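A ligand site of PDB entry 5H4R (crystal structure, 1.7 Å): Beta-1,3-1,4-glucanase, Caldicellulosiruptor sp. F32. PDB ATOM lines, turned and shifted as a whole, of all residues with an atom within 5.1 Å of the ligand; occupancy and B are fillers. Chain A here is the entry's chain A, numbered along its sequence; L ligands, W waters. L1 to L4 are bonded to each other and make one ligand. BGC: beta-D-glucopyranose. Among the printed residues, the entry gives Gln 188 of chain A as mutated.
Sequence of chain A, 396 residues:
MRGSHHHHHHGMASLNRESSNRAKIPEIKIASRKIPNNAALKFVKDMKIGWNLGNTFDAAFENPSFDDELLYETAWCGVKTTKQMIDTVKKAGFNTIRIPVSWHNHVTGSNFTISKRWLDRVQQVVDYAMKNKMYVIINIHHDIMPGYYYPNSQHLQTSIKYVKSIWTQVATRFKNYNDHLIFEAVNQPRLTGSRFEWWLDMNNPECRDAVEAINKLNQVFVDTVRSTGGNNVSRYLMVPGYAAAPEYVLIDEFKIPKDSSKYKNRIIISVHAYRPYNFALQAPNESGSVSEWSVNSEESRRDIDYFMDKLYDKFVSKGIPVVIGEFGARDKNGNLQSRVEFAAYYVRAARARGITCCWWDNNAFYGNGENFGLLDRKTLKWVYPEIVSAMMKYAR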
ATOM      1  N   ASN A  55     -21.327  -4.365   1.312  1.00  0.00           N
ATOM      2  CA  ASN A  55     -21.437  -5.830   1.393  1.00  0.00           C
ATOM      3  C   ASN A  55     -20.662  -6.404   2.582  1.00  0.00           C
ATOM      4  O   ASN A  55     -20.104  -7.508   2.516  1.00  0.00           O
ATOM      5  CB  ASN A  55     -20.979  -6.479   0.079  1.00  0.00           C
ATOM      6  CG  ASN A  55     -22.097  -6.476  -0.987  1.00  0.00           C
ATOM      7  OD1 ASN A  55     -23.140  -5.859  -0.815  1.00  0.00           O
ATOM      8  ND2 ASN A  55     -21.860  -7.184  -2.083  1.00  0.00           N
ATOM      9  N   ASP A  58     -23.745  -5.033   6.232  1.00  0.00           N
ATOM     10  CA  ASP A  58     -25.052  -5.006   5.571  1.00  0.00           C
ATOM     11  C   ASP A  58     -25.476  -6.350   4.992  1.00  0.00           C
ATOM     12  O   ASP A  58     -26.646  -6.510   4.612  1.00  0.00           O
ATOM     13  CB  ASP A  58     -25.091  -3.950   4.458  1.00  0.00           C
ATOM     14  CG  ASP A  58     -23.833  -3.925   3.580  1.00  0.00           C
ATOM     15  OD1 ASP A  58     -22.693  -3.891   4.111  1.00  0.00           O
ATOM     16  OD2 ASP A  58     -24.002  -3.922   2.342  1.00  0.00           O
ATOM     17  N   TRP A  76     -20.354 -11.901   2.290  1.00  0.00           N
ATOM     18  CA  TRP A  76     -20.405 -11.362   0.945  1.00  0.00           C
ATOM     19  C   TRP A  76     -19.052 -10.812   0.480  1.00  0.00           C
ATOM     20  O   TRP A  76     -18.613 -11.149  -0.617  1.00  0.00           O
ATOM     21  CB  TRP A  76     -21.491 -10.283   0.842  1.00  0.00           C
ATOM     22  CG  TRP A  76     -22.919 -10.821   0.934  1.00  0.00           C
ATOM     23  CD1 TRP A  76     -23.314 -12.115   1.066  1.00  0.00           C
ATOM     24  CD2 TRP A  76     -24.118 -10.035   0.907  1.00  0.00           C
ATOM     25  NE1 TRP A  76     -24.682 -12.201   1.103  1.00  0.00           N
ATOM     26  CE2 TRP A  76     -25.210 -10.930   1.019  1.00  0.00           C
ATOM     27  CE3 TRP A  76     -24.378  -8.661   0.809  1.00  0.00           C
ATOM     28  CZ2 TRP A  76     -26.525 -10.500   1.031  1.00  0.00           C
ATOM     29  CZ3 TRP A  76     -25.687  -8.238   0.821  1.00  0.00           C
ATOM     30  CH2 TRP A  76     -26.746  -9.146   0.924  1.00  0.00           C
ATOM     31  N   HIS A 141     -29.833  -0.947   7.270  1.00  0.00           N
ATOM     32  CA  HIS A 141     -29.669  -1.201   5.844  1.00  0.00           C
ATOM     33  C   HIS A 141     -30.714  -2.209   5.359  1.00  0.00           C
ATOM     34  O   HIS A 141     -31.883  -1.816   5.145  1.00  0.00           O
ATOM     35  CB  HIS A 141     -28.215  -1.599   5.571  1.00  0.00           C
ATOM     36  CG  HIS A 141     -27.787  -1.273   4.180  1.00  0.00           C
ATOM     37  ND1 HIS A 141     -27.437   0.009   3.788  1.00  0.00           N
ATOM     38  CD2 HIS A 141     -27.676  -2.054   3.074  1.00  0.00           C
ATOM     39  CE1 HIS A 141     -27.112  -0.010   2.510  1.00  0.00           C
ATOM     40  NE2 HIS A 141     -27.229  -1.249   2.061  1.00  0.00           N
ATOM     41  N   HIS A 142     -30.359  -3.480   5.124  1.00  0.00           N
ATOM     42  CA  HIS A 142     -31.255  -4.459   4.487  1.00  0.00           C
ATOM     43  C   HIS A 142     -32.186  -5.101   5.515  1.00  0.00           C
ATOM     44  O   HIS A 142     -32.207  -6.324   5.687  1.00  0.00           O
ATOM     45  CB  HIS A 142     -30.509  -5.561   3.751  1.00  0.00           C
ATOM     46  CG  HIS A 142     -29.703  -5.133   2.581  1.00  0.00           C
ATOM     47  ND1 HIS A 142     -30.195  -4.334   1.562  1.00  0.00           N
ATOM     48  CD2 HIS A 142     -28.425  -5.431   2.234  1.00  0.00           C
ATOM     49  CE1 HIS A 142     -29.247  -4.146   0.652  1.00  0.00           C
ATOM     50  NE2 HIS A 142     -28.169  -4.812   1.032  1.00  0.00           N
ATOM     51  N   ASN A 187     -31.819   2.980   5.113  1.00  0.00           N
ATOM     52  CA  ASN A 187     -31.151   3.036   3.826  1.00  0.00           C
ATOM     53  C   ASN A 187     -32.101   3.395   2.696  1.00  0.00           C
ATOM     54  O   ASN A 187     -32.108   4.534   2.223  1.00  0.00           O
ATOM     55  CB  ASN A 187     -30.456   1.692   3.595  1.00  0.00           C
ATOM     56  CG  ASN A 187     -29.790   1.596   2.284  1.00  0.00           C
ATOM     57  OD1 ASN A 187     -29.027   2.481   1.911  1.00  0.00           O
ATOM     58  ND2 ASN A 187     -30.031   0.504   1.570  1.00  0.00           N
ATOM     59  N   GLN A 188     -32.931   2.451   2.258  1.00  0.00           N
ATOM     60  CA  GLN A 188     -33.798   2.635   1.089  1.00  0.00           C
ATOM     61  C   GLN A 188     -35.207   2.156   1.451  1.00  0.00           C
ATOM     62  O   GLN A 188     -35.676   1.111   0.984  1.00  0.00           O
ATOM     63  CB  GLN A 188     -33.253   1.928  -0.145  1.00  0.00           C
ATOM     64  CG  GLN A 188     -31.977   2.559  -0.593  1.00  0.00           C
ATOM     65  CD  GLN A 188     -31.377   2.019  -1.851  1.00  0.00           C
ATOM     66  OE1 GLN A 188     -30.683   2.753  -2.555  1.00  0.00           O
ATOM     67  NE2 GLN A 188     -31.569   0.726  -2.120  1.00  0.00           N
ATOM     68  N   TRP A 198     -39.584   0.564  -6.607  1.00  0.00           N
ATOM     69  CA  TRP A 198     -38.627   1.580  -7.000  1.00  0.00           C
ATOM     70  C   TRP A 198     -39.249   2.802  -7.662  1.00  0.00           C
ATOM     71  O   TRP A 198     -38.511   3.696  -8.104  1.00  0.00           O
ATOM     72  CB  TRP A 198     -37.569   0.995  -7.952  1.00  0.00           C
ATOM     73  CG  TRP A 198     -36.842  -0.182  -7.341  1.00  0.00           C
ATOM     74  CD1 TRP A 198     -36.979  -1.493  -7.702  1.00  0.00           C
ATOM     75  CD2 TRP A 198     -35.917  -0.162  -6.245  1.00  0.00           C
ATOM     76  NE1 TRP A 198     -36.161  -2.279  -6.925  1.00  0.00           N
ATOM     77  CE2 TRP A 198     -35.524  -1.490  -5.999  1.00  0.00           C
ATOM     78  CE3 TRP A 198     -35.387   0.851  -5.437  1.00  0.00           C
ATOM     79  CZ2 TRP A 198     -34.603  -1.842  -5.011  1.00  0.00           C
ATOM     80  CZ3 TRP A 198     -34.482   0.502  -4.429  1.00  0.00           C
ATOM     81  CH2 TRP A 198     -34.090  -0.835  -4.241  1.00  0.00           C
ATOM     82  N   ALA A 243     -37.232   4.947  -1.104  1.00  0.00           N
ATOM     83  CA  ALA A 243     -36.187   4.260  -1.851  1.00  0.00           C
ATOM     84  C   ALA A 243     -34.882   5.046  -1.890  1.00  0.00           C
ATOM     85  O   ALA A 243     -33.981   4.711  -2.672  1.00  0.00           O
ATOM     86  CB  ALA A 243     -36.652   3.916  -3.271  1.00  0.00           C
ATOM     87  N   HIS A 272     -29.595   8.393  -2.812  1.00  0.00           N
ATOM     88  CA  HIS A 272     -28.742   7.489  -3.590  1.00  0.00           C
ATOM     89  C   HIS A 272     -29.051   7.711  -5.052  1.00  0.00           C
ATOM     90  O   HIS A 272     -30.211   7.915  -5.411  1.00  0.00           O
ATOM     91  CB  HIS A 272     -28.996   6.041  -3.248  1.00  0.00           C
ATOM     92  CG  HIS A 272     -28.725   5.711  -1.831  1.00  0.00           C
ATOM     93  ND1 HIS A 272     -29.028   4.493  -1.286  1.00  0.00           N
ATOM     94  CD2 HIS A 272     -28.209   6.469  -0.842  1.00  0.00           C
ATOM     95  CE1 HIS A 272     -28.686   4.504  -0.002  1.00  0.00           C
ATOM     96  NE2 HIS A 272     -28.171   5.684   0.289  1.00  0.00           N
ATOM     97  N   TYR A 274     -27.419   6.182  -8.645  1.00  0.00           N
ATOM     98  CA  TYR A 274     -26.533   5.511  -9.601  1.00  0.00           C
ATOM     99  C   TYR A 274     -27.040   5.878 -10.988  1.00  0.00           C
ATOM    100  O   TYR A 274     -27.818   5.157 -11.608  1.00  0.00           O
ATOM    101  CB  TYR A 274     -26.531   4.020  -9.371  1.00  0.00           C
ATOM    102  CG  TYR A 274     -26.056   3.525  -8.020  1.00  0.00           C
ATOM    103  CD1 TYR A 274     -26.893   3.492  -6.915  1.00  0.00           C
ATOM    104  CD2 TYR A 274     -24.795   3.015  -7.870  1.00  0.00           C
ATOM    105  CE1 TYR A 274     -26.465   3.003  -5.694  1.00  0.00           C
ATOM    106  CE2 TYR A 274     -24.359   2.490  -6.670  1.00  0.00           C
ATOM    107  CZ  TYR A 274     -25.183   2.495  -5.569  1.00  0.00           C
ATOM    108  OH  TYR A 274     -24.754   1.961  -4.385  1.00  0.00           O
ATOM    109  N   TYR A 277     -28.692   5.426 -14.983  1.00  0.00           N
ATOM    110  CA  TYR A 277     -28.874   4.041 -14.562  1.00  0.00           C
ATOM    111  C   TYR A 277     -28.327   3.044 -15.577  1.00  0.00           C
ATOM    112  O   TYR A 277     -27.658   2.064 -15.204  1.00  0.00           O
ATOM    113  CB  TYR A 277     -30.363   3.798 -14.312  1.00  0.00           C
ATOM    114  CG  TYR A 277     -30.732   2.352 -14.091  1.00  0.00           C
ATOM    115  CD1 TYR A 277     -30.524   1.749 -12.848  1.00  0.00           C
ATOM    116  CD2 TYR A 277     -31.260   1.592 -15.112  1.00  0.00           C
ATOM    117  CE1 TYR A 277     -30.839   0.440 -12.659  1.00  0.00           C
ATOM    118  CE2 TYR A 277     -31.571   0.276 -14.907  1.00  0.00           C
ATOM    119  CZ  TYR A 277     -31.364  -0.290 -13.685  1.00  0.00           C
ATOM    120  OH  TYR A 277     -31.701  -1.634 -13.515  1.00  0.00           O
ATOM    121  N   LEU A 281     -25.536   1.238 -13.192  1.00  0.00           N
ATOM    122  CA  LEU A 281     -26.064   0.205 -12.319  1.00  0.00           C
ATOM    123  C   LEU A 281     -26.716  -0.951 -13.072  1.00  0.00           C
ATOM    124  O   LEU A 281     -26.620  -2.095 -12.626  1.00  0.00           O
ATOM    125  CB  LEU A 281     -27.054   0.839 -11.353  1.00  0.00           C
ATOM    126  CG  LEU A 281     -27.787  -0.096 -10.401  1.00  0.00           C
ATOM    127  CD1 LEU A 281     -26.818  -0.842  -9.531  1.00  0.00           C
ATOM    128  CD2 LEU A 281     -28.750   0.734  -9.550  1.00  0.00           C
ATOM    129  N   GLU A 326     -24.715   7.018  -1.593  1.00  0.00           N
ATOM    130  CA  GLU A 326     -24.251   5.949  -2.487  1.00  0.00           C
ATOM    131  C   GLU A 326     -24.346   6.420  -3.935  1.00  0.00           C
ATOM    132  O   GLU A 326     -25.385   6.926  -4.354  1.00  0.00           O
ATOM    133  CB  GLU A 326     -25.088   4.662  -2.371  1.00  0.00           C
ATOM    134  CG  GLU A 326     -25.022   3.944  -1.054  1.00  0.00           C
ATOM    135  CD  GLU A 326     -25.887   2.686  -1.029  1.00  0.00           C
ATOM    136  OE1 GLU A 326     -26.205   2.144  -2.116  1.00  0.00           O
ATOM    137  OE2 GLU A 326     -26.262   2.245   0.089  1.00  0.00           O
ATOM    138  N   TRP A 360     -19.927   3.434  -3.586  1.00  0.00           N
ATOM    139  CA  TRP A 360     -20.315   2.107  -3.087  1.00  0.00           C
ATOM    140  C   TRP A 360     -19.215   1.108  -3.440  1.00  0.00           C
ATOM    141  O   TRP A 360     -19.115   0.676  -4.593  1.00  0.00           O
ATOM    142  CB  TRP A 360     -21.644   1.699  -3.722  1.00  0.00           C
ATOM    143  CG  TRP A 360     -22.128   0.372  -3.277  1.00  0.00           C
ATOM    144  CD1 TRP A 360     -22.166  -0.769  -3.998  1.00  0.00           C
ATOM    145  CD2 TRP A 360     -22.598   0.048  -1.980  1.00  0.00           C
ATOM    146  NE1 TRP A 360     -22.658  -1.799  -3.233  1.00  0.00           N
ATOM    147  CE2 TRP A 360     -22.928  -1.329  -1.981  1.00  0.00           C
ATOM    148  CE3 TRP A 360     -22.792   0.778  -0.804  1.00  0.00           C
ATOM    149  CZ2 TRP A 360     -23.444  -1.965  -0.870  1.00  0.00           C
ATOM    150  CZ3 TRP A 360     -23.315   0.133   0.292  1.00  0.00           C
ATOM    151  CH2 TRP A 360     -23.631  -1.222   0.257  1.00  0.00           C
ATOM    152  N   ASN A 362     -18.131  -2.488  -2.808  1.00  0.00           N
ATOM    153  CA  ASN A 362     -18.564  -3.772  -2.288  1.00  0.00           C
ATOM    154  C   ASN A 362     -17.514  -4.882  -2.451  1.00  0.00           C
ATOM    155  O   ASN A 362     -17.847  -6.057  -2.256  1.00  0.00           O
ATOM    156  CB  ASN A 362     -19.896  -4.184  -2.931  1.00  0.00           C
ATOM    157  CG  ASN A 362     -19.767  -4.450  -4.421  1.00  0.00           C
ATOM    158  OD1 ASN A 362     -18.746  -4.165  -5.022  1.00  0.00           O
ATOM    159  ND2 ASN A 362     -20.805  -5.011  -5.021  1.00  0.00           N
ATOM    160  N   GLU A 370     -22.489  -7.425  -9.022  1.00  0.00           N
ATOM    161  CA  GLU A 370     -22.356  -5.982  -9.213  1.00  0.00           C
ATOM    162  C   GLU A 370     -20.925  -5.581  -8.875  1.00  0.00           C
ATOM    163  O   GLU A 370     -20.573  -5.430  -7.702  1.00  0.00           O
ATOM    164  CB  GLU A 370     -23.357  -5.240  -8.356  1.00  0.00           C
ATOM    165  CG  GLU A 370     -24.782  -5.627  -8.643  1.00  0.00           C
ATOM    166  CD  GLU A 370     -25.821  -4.893  -7.800  1.00  0.00           C
ATOM    167  OE1 GLU A 370     -25.427  -4.016  -6.997  1.00  0.00           O
ATOM    168  OE2 GLU A 370     -27.026  -5.212  -7.945  1.00  0.00           O
ATOM    169  N   PHE A 372     -18.568  -3.258  -8.276  1.00  0.00           N
ATOM    170  CA  PHE A 372     -18.352  -1.883  -7.878  1.00  0.00           C
ATOM    171  C   PHE A 372     -17.038  -1.687  -7.111  1.00  0.00           C
ATOM    172  O   PHE A 372     -16.762  -0.576  -6.664  1.00  0.00           O
ATOM    173  CB  PHE A 372     -19.515  -1.415  -6.983  1.00  0.00           C
ATOM    174  CG  PHE A 372     -20.789  -1.060  -7.727  1.00  0.00           C
ATOM    175  CD1 PHE A 372     -20.870   0.126  -8.442  1.00  0.00           C
ATOM    176  CD2 PHE A 372     -21.920  -1.857  -7.628  1.00  0.00           C
ATOM    177  CE1 PHE A 372     -22.038   0.483  -9.088  1.00  0.00           C
ATOM    178  CE2 PHE A 372     -23.107  -1.502  -8.263  1.00  0.00           C
ATOM    179  CZ  PHE A 372     -23.147  -0.324  -9.007  1.00  0.00           C
HETATM  180  C2  BGC L   1     -30.994  -1.524  -7.102  1.00  0.00           C
HETATM  181  C3  BGC L   1     -30.508  -1.712  -5.658  1.00  0.00           C
HETATM  182  C4  BGC L   1     -29.736  -0.478  -5.198  1.00  0.00           C
HETATM  183  C5  BGC L   1     -30.594   0.776  -5.400  1.00  0.00           C
HETATM  184  C6  BGC L   1     -29.859   2.110  -5.318  1.00  0.00           C
HETATM  185  C1  BGC L   1     -31.850  -0.264  -7.196  1.00  0.00           C
HETATM  186  O1  BGC L   1     -32.248   0.030  -8.544  1.00  0.00           O
HETATM  187  O2  BGC L   1     -31.727  -2.694  -7.469  1.00  0.00           O
HETATM  188  O3  BGC L   1     -29.663  -2.862  -5.586  1.00  0.00           O
HETATM  189  O4  BGC L   1     -29.442  -0.752  -3.811  1.00  0.00           O
HETATM  190  O5  BGC L   1     -31.036   0.802  -6.745  1.00  0.00           O
HETATM  191  O6  BGC L   1     -30.711   3.199  -5.766  1.00  0.00           O
HETATM  192  C2  BGC L   2     -28.184  -0.545  -1.818  1.00  0.00           C
HETATM  193  C3  BGC L   2     -26.885  -1.343  -1.745  1.00  0.00           C
HETATM  194  C4  BGC L   2     -26.690  -2.003  -3.099  1.00  0.00           C
HETATM  195  C5  BGC L   2     -26.304  -0.865  -4.040  1.00  0.00           C
HETATM  196  C6  BGC L   2     -26.074  -1.357  -5.472  1.00  0.00           C
HETATM  197  C1  BGC L   2     -28.446   0.083  -3.201  1.00  0.00           C
HETATM  198  O2  BGC L   2     -28.208   0.439  -0.773  1.00  0.00           O
HETATM  199  O3  BGC L   2     -27.039  -2.300  -0.709  1.00  0.00           O
HETATM  200  O4  BGC L   2     -25.608  -2.922  -2.988  1.00  0.00           O
HETATM  201  O5  BGC L   2     -27.299   0.160  -4.055  1.00  0.00           O
HETATM  202  O6  BGC L   2     -27.151  -2.156  -5.989  1.00  0.00           O
HETATM  203  C2  BGC L   3     -24.525  -4.880  -3.791  1.00  0.00           C
HETATM  204  C3  BGC L   3     -24.771  -6.276  -4.338  1.00  0.00           C
HETATM  205  C4  BGC L   3     -25.670  -7.046  -3.363  1.00  0.00           C
HETATM  206  C5  BGC L   3     -26.947  -6.243  -3.073  1.00  0.00           C
HETATM  207  C6  BGC L   3     -27.810  -6.901  -2.017  1.00  0.00           C
HETATM  208  C1  BGC L   3     -25.866  -4.196  -3.550  1.00  0.00           C
HETATM  209  O2  BGC L   3     -23.741  -4.141  -4.730  1.00  0.00           O
HETATM  210  O3  BGC L   3     -23.495  -6.910  -4.475  1.00  0.00           O
HETATM  211  O4  BGC L   3     -26.077  -8.241  -4.037  1.00  0.00           O
HETATM  212  O5  BGC L   3     -26.597  -4.966  -2.595  1.00  0.00           O
HETATM  213  O6  BGC L   3     -29.100  -6.229  -1.983  1.00  0.00           O
HETATM  214  C2  BGC L   4     -26.635 -10.552  -4.036  1.00  0.00           C
HETATM  215  C3  BGC L   4     -26.405 -11.908  -3.367  1.00  0.00           C
HETATM  216  C4  BGC L   4     -24.922 -12.149  -3.295  1.00  0.00           C
HETATM  217  C5  BGC L   4     -24.218 -10.946  -2.632  1.00  0.00           C
HETATM  218  C6  BGC L   4     -22.725 -11.173  -2.522  1.00  0.00           C
HETATM  219  C1  BGC L   4     -25.830  -9.443  -3.341  1.00  0.00           C
HETATM  220  O2  BGC L   4     -28.028 -10.287  -3.940  1.00  0.00           O
HETATM  221  O3  BGC L   4     -27.030 -12.938  -4.158  1.00  0.00           O
HETATM  222  O4  BGC L   4     -24.743 -13.318  -2.511  1.00  0.00           O
HETATM  223  O5  BGC L   4     -24.458  -9.781  -3.435  1.00  0.00           O
HETATM  224  O6  BGC L   4     -22.220 -11.334  -3.841  1.00  0.00           O
HETATM  225  O   HOH W   1     -26.666 -15.697  -2.371  1.00  0.00           O
HETATM  226  O   HOH W   2     -29.593 -10.446  -1.654  1.00  0.00           O
HETATM  227  O   HOH W   3     -29.341  -8.427  -5.330  1.00  0.00           O
HETATM  228  O   HOH W   4     -26.550 -14.327   0.063  1.00  0.00           O
HETATM  229  O   HOH W   5     -28.966  -5.578  -6.248  1.00  0.00           O
HETATM  230  O   HOH W   6     -19.545 -12.699  -2.700  1.00  0.00           O
HETATM  231  O   HOH W   7     -30.255  -3.729  -2.932  1.00  0.00           O
HETATM  232  O   HOH W   8     -30.503  -7.548  -0.116  1.00  0.00           O
HETATM  233  O   HOH W   9     -23.528  -8.678  -6.541  1.00  0.00           O
HETATM  234  O   HOH W  10     -25.519  -4.536   0.260  1.00  0.00           O
HETATM  235  O   HOH W  11     -20.770  -9.546  -4.838  1.00  0.00           O
HETATM  236  O   HOH W  12     -29.362 -13.205  -3.069  1.00  0.00           O
HETATM  237  O   HOH W  13     -33.174   4.812  -5.234  1.00  0.00           O
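O2 of BGC L3 lies within hydrogen-bond range of NE1 of Trp 360, 3.0 Å away.
A ring nitrogen (NE2) of His 141 lies within hydrogen-bond range of an oxygen (O3) of BGC L2.
OE2 of Glu 326 is in hydrogen-bond range of O2 of BGC L2 (2.8 Å).
The side-chain amide nitrogen of Gln 188 lies within hydrogen-bond range of an oxygen (O4) of BGC L1.
ND2 of Asn 187 is in hydrogen-bond range of O2 of BGC L2, 3.0 Å away.
ND2 of Asn 362 sits at hydrogen-bond distance from O2 of BGC L3 (3.1 Å).
OE1 of Glu 370 lies within hydrogen-bond range of O6 of BGC L2, 2.7 Å away.
OH of Tyr 274 sits at hydrogen-bond distance from O5 of BGC L2, 3.1 Å away.
The side-chain amide nitrogen (ND2) of Asn 55 is in hydrogen-bond range of an oxygen (O3) of BGC L3, at 2.9 Å.
A ring nitrogen (NE2) of His 142 lies close to an oxygen (O3) of BGC L2, at 3.3 Å.
Water W9 lies within hydrogen-bond range of an oxygen (O3) of BGC L3 and the backbone NH (N) of Glu 370.
Water W10 lies within hydrogen-bond range of the side-chain carboxylate (OD2) of Asp 58 (2.6 Å), a ring nitrogen (NE2) of His 142 (2.8 Å), an oxygen (O3) of BGC L2 (2.9 Å) and the side-chain amide oxygen (OD1) of Asn 55 (2.9 Å).
Water W5 bridges the side-chain carboxylate of Glu 370 and an oxygen (O3) of BGC L1.
Water W13 lies within hydrogen-bond range of O of Ala 243 (2.7 Å) and O6 of BGC L1 (3.0 Å).
Water W6 bridges O of Trp 76 (2.8 Å) and O6 of BGC L4 (3.2 Å).
Water W4 bridges the indole nitrogen (NE1) of Trp 76 (3.0 Å) and an oxygen (O4) of BGC L4 (3.3 Å).
CG of Trp 76 touches C6 of BGC L4, at 3.5 Å.
CH2 of Trp 198 touches C1 of BGC L1 (3.8 Å).
Leu 281 touches the ligand.
Hydrophobic or aromatic side chains within 4 Å of the ligand: Trp 76, His 141, His 142, Trp 198, Tyr 274, Leu 281 and Trp 360.
Within 4 Å of the ligand: Asn 55, Trp 76, His 141, His 142, Asn 187, Gln 188, Trp 198, Tyr 274, Leu 281, Glu 326, Trp 360, Asn 362 and Glu 370.
The nearest printed residue that does not touch the ligand is Phe 372 (4.1 Å).
The side-chain hydroxyl (OH) of Tyr 274 lies within hydrogen-bond range of the side-chain carboxylate (OE1) of Glu 326, 2.7 Å away.
The side-chain amide nitrogen (ND2) of Asn 362 lies within hydrogen-bond range of the backbone carbonyl oxygen (O) of Glu 370 (2.7 Å).
The side-chain amide oxygen (OD1) of Asn 362 is in hydrogen-bond range of the backbone NH (N) of Phe 372.
NE2 of His 141 lies close to ND2 of Asn 187 (3.3 Å).
The backbone NH (N) of Asn 55 is in hydrogen-bond range of the side-chain carboxylate (OD2) of Asp 58 (2.9 Å).
The side-chain amide oxygen (OD1) of Asn 187 sits close to the side-chain carboxylate (OE2) of Glu 326 (3.3 Å).
A ring nitrogen (ND1) of His 272 lies within hydrogen-bond range of the side-chain amide oxygen (OE1) of Gln 188, 2.7 Å away.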
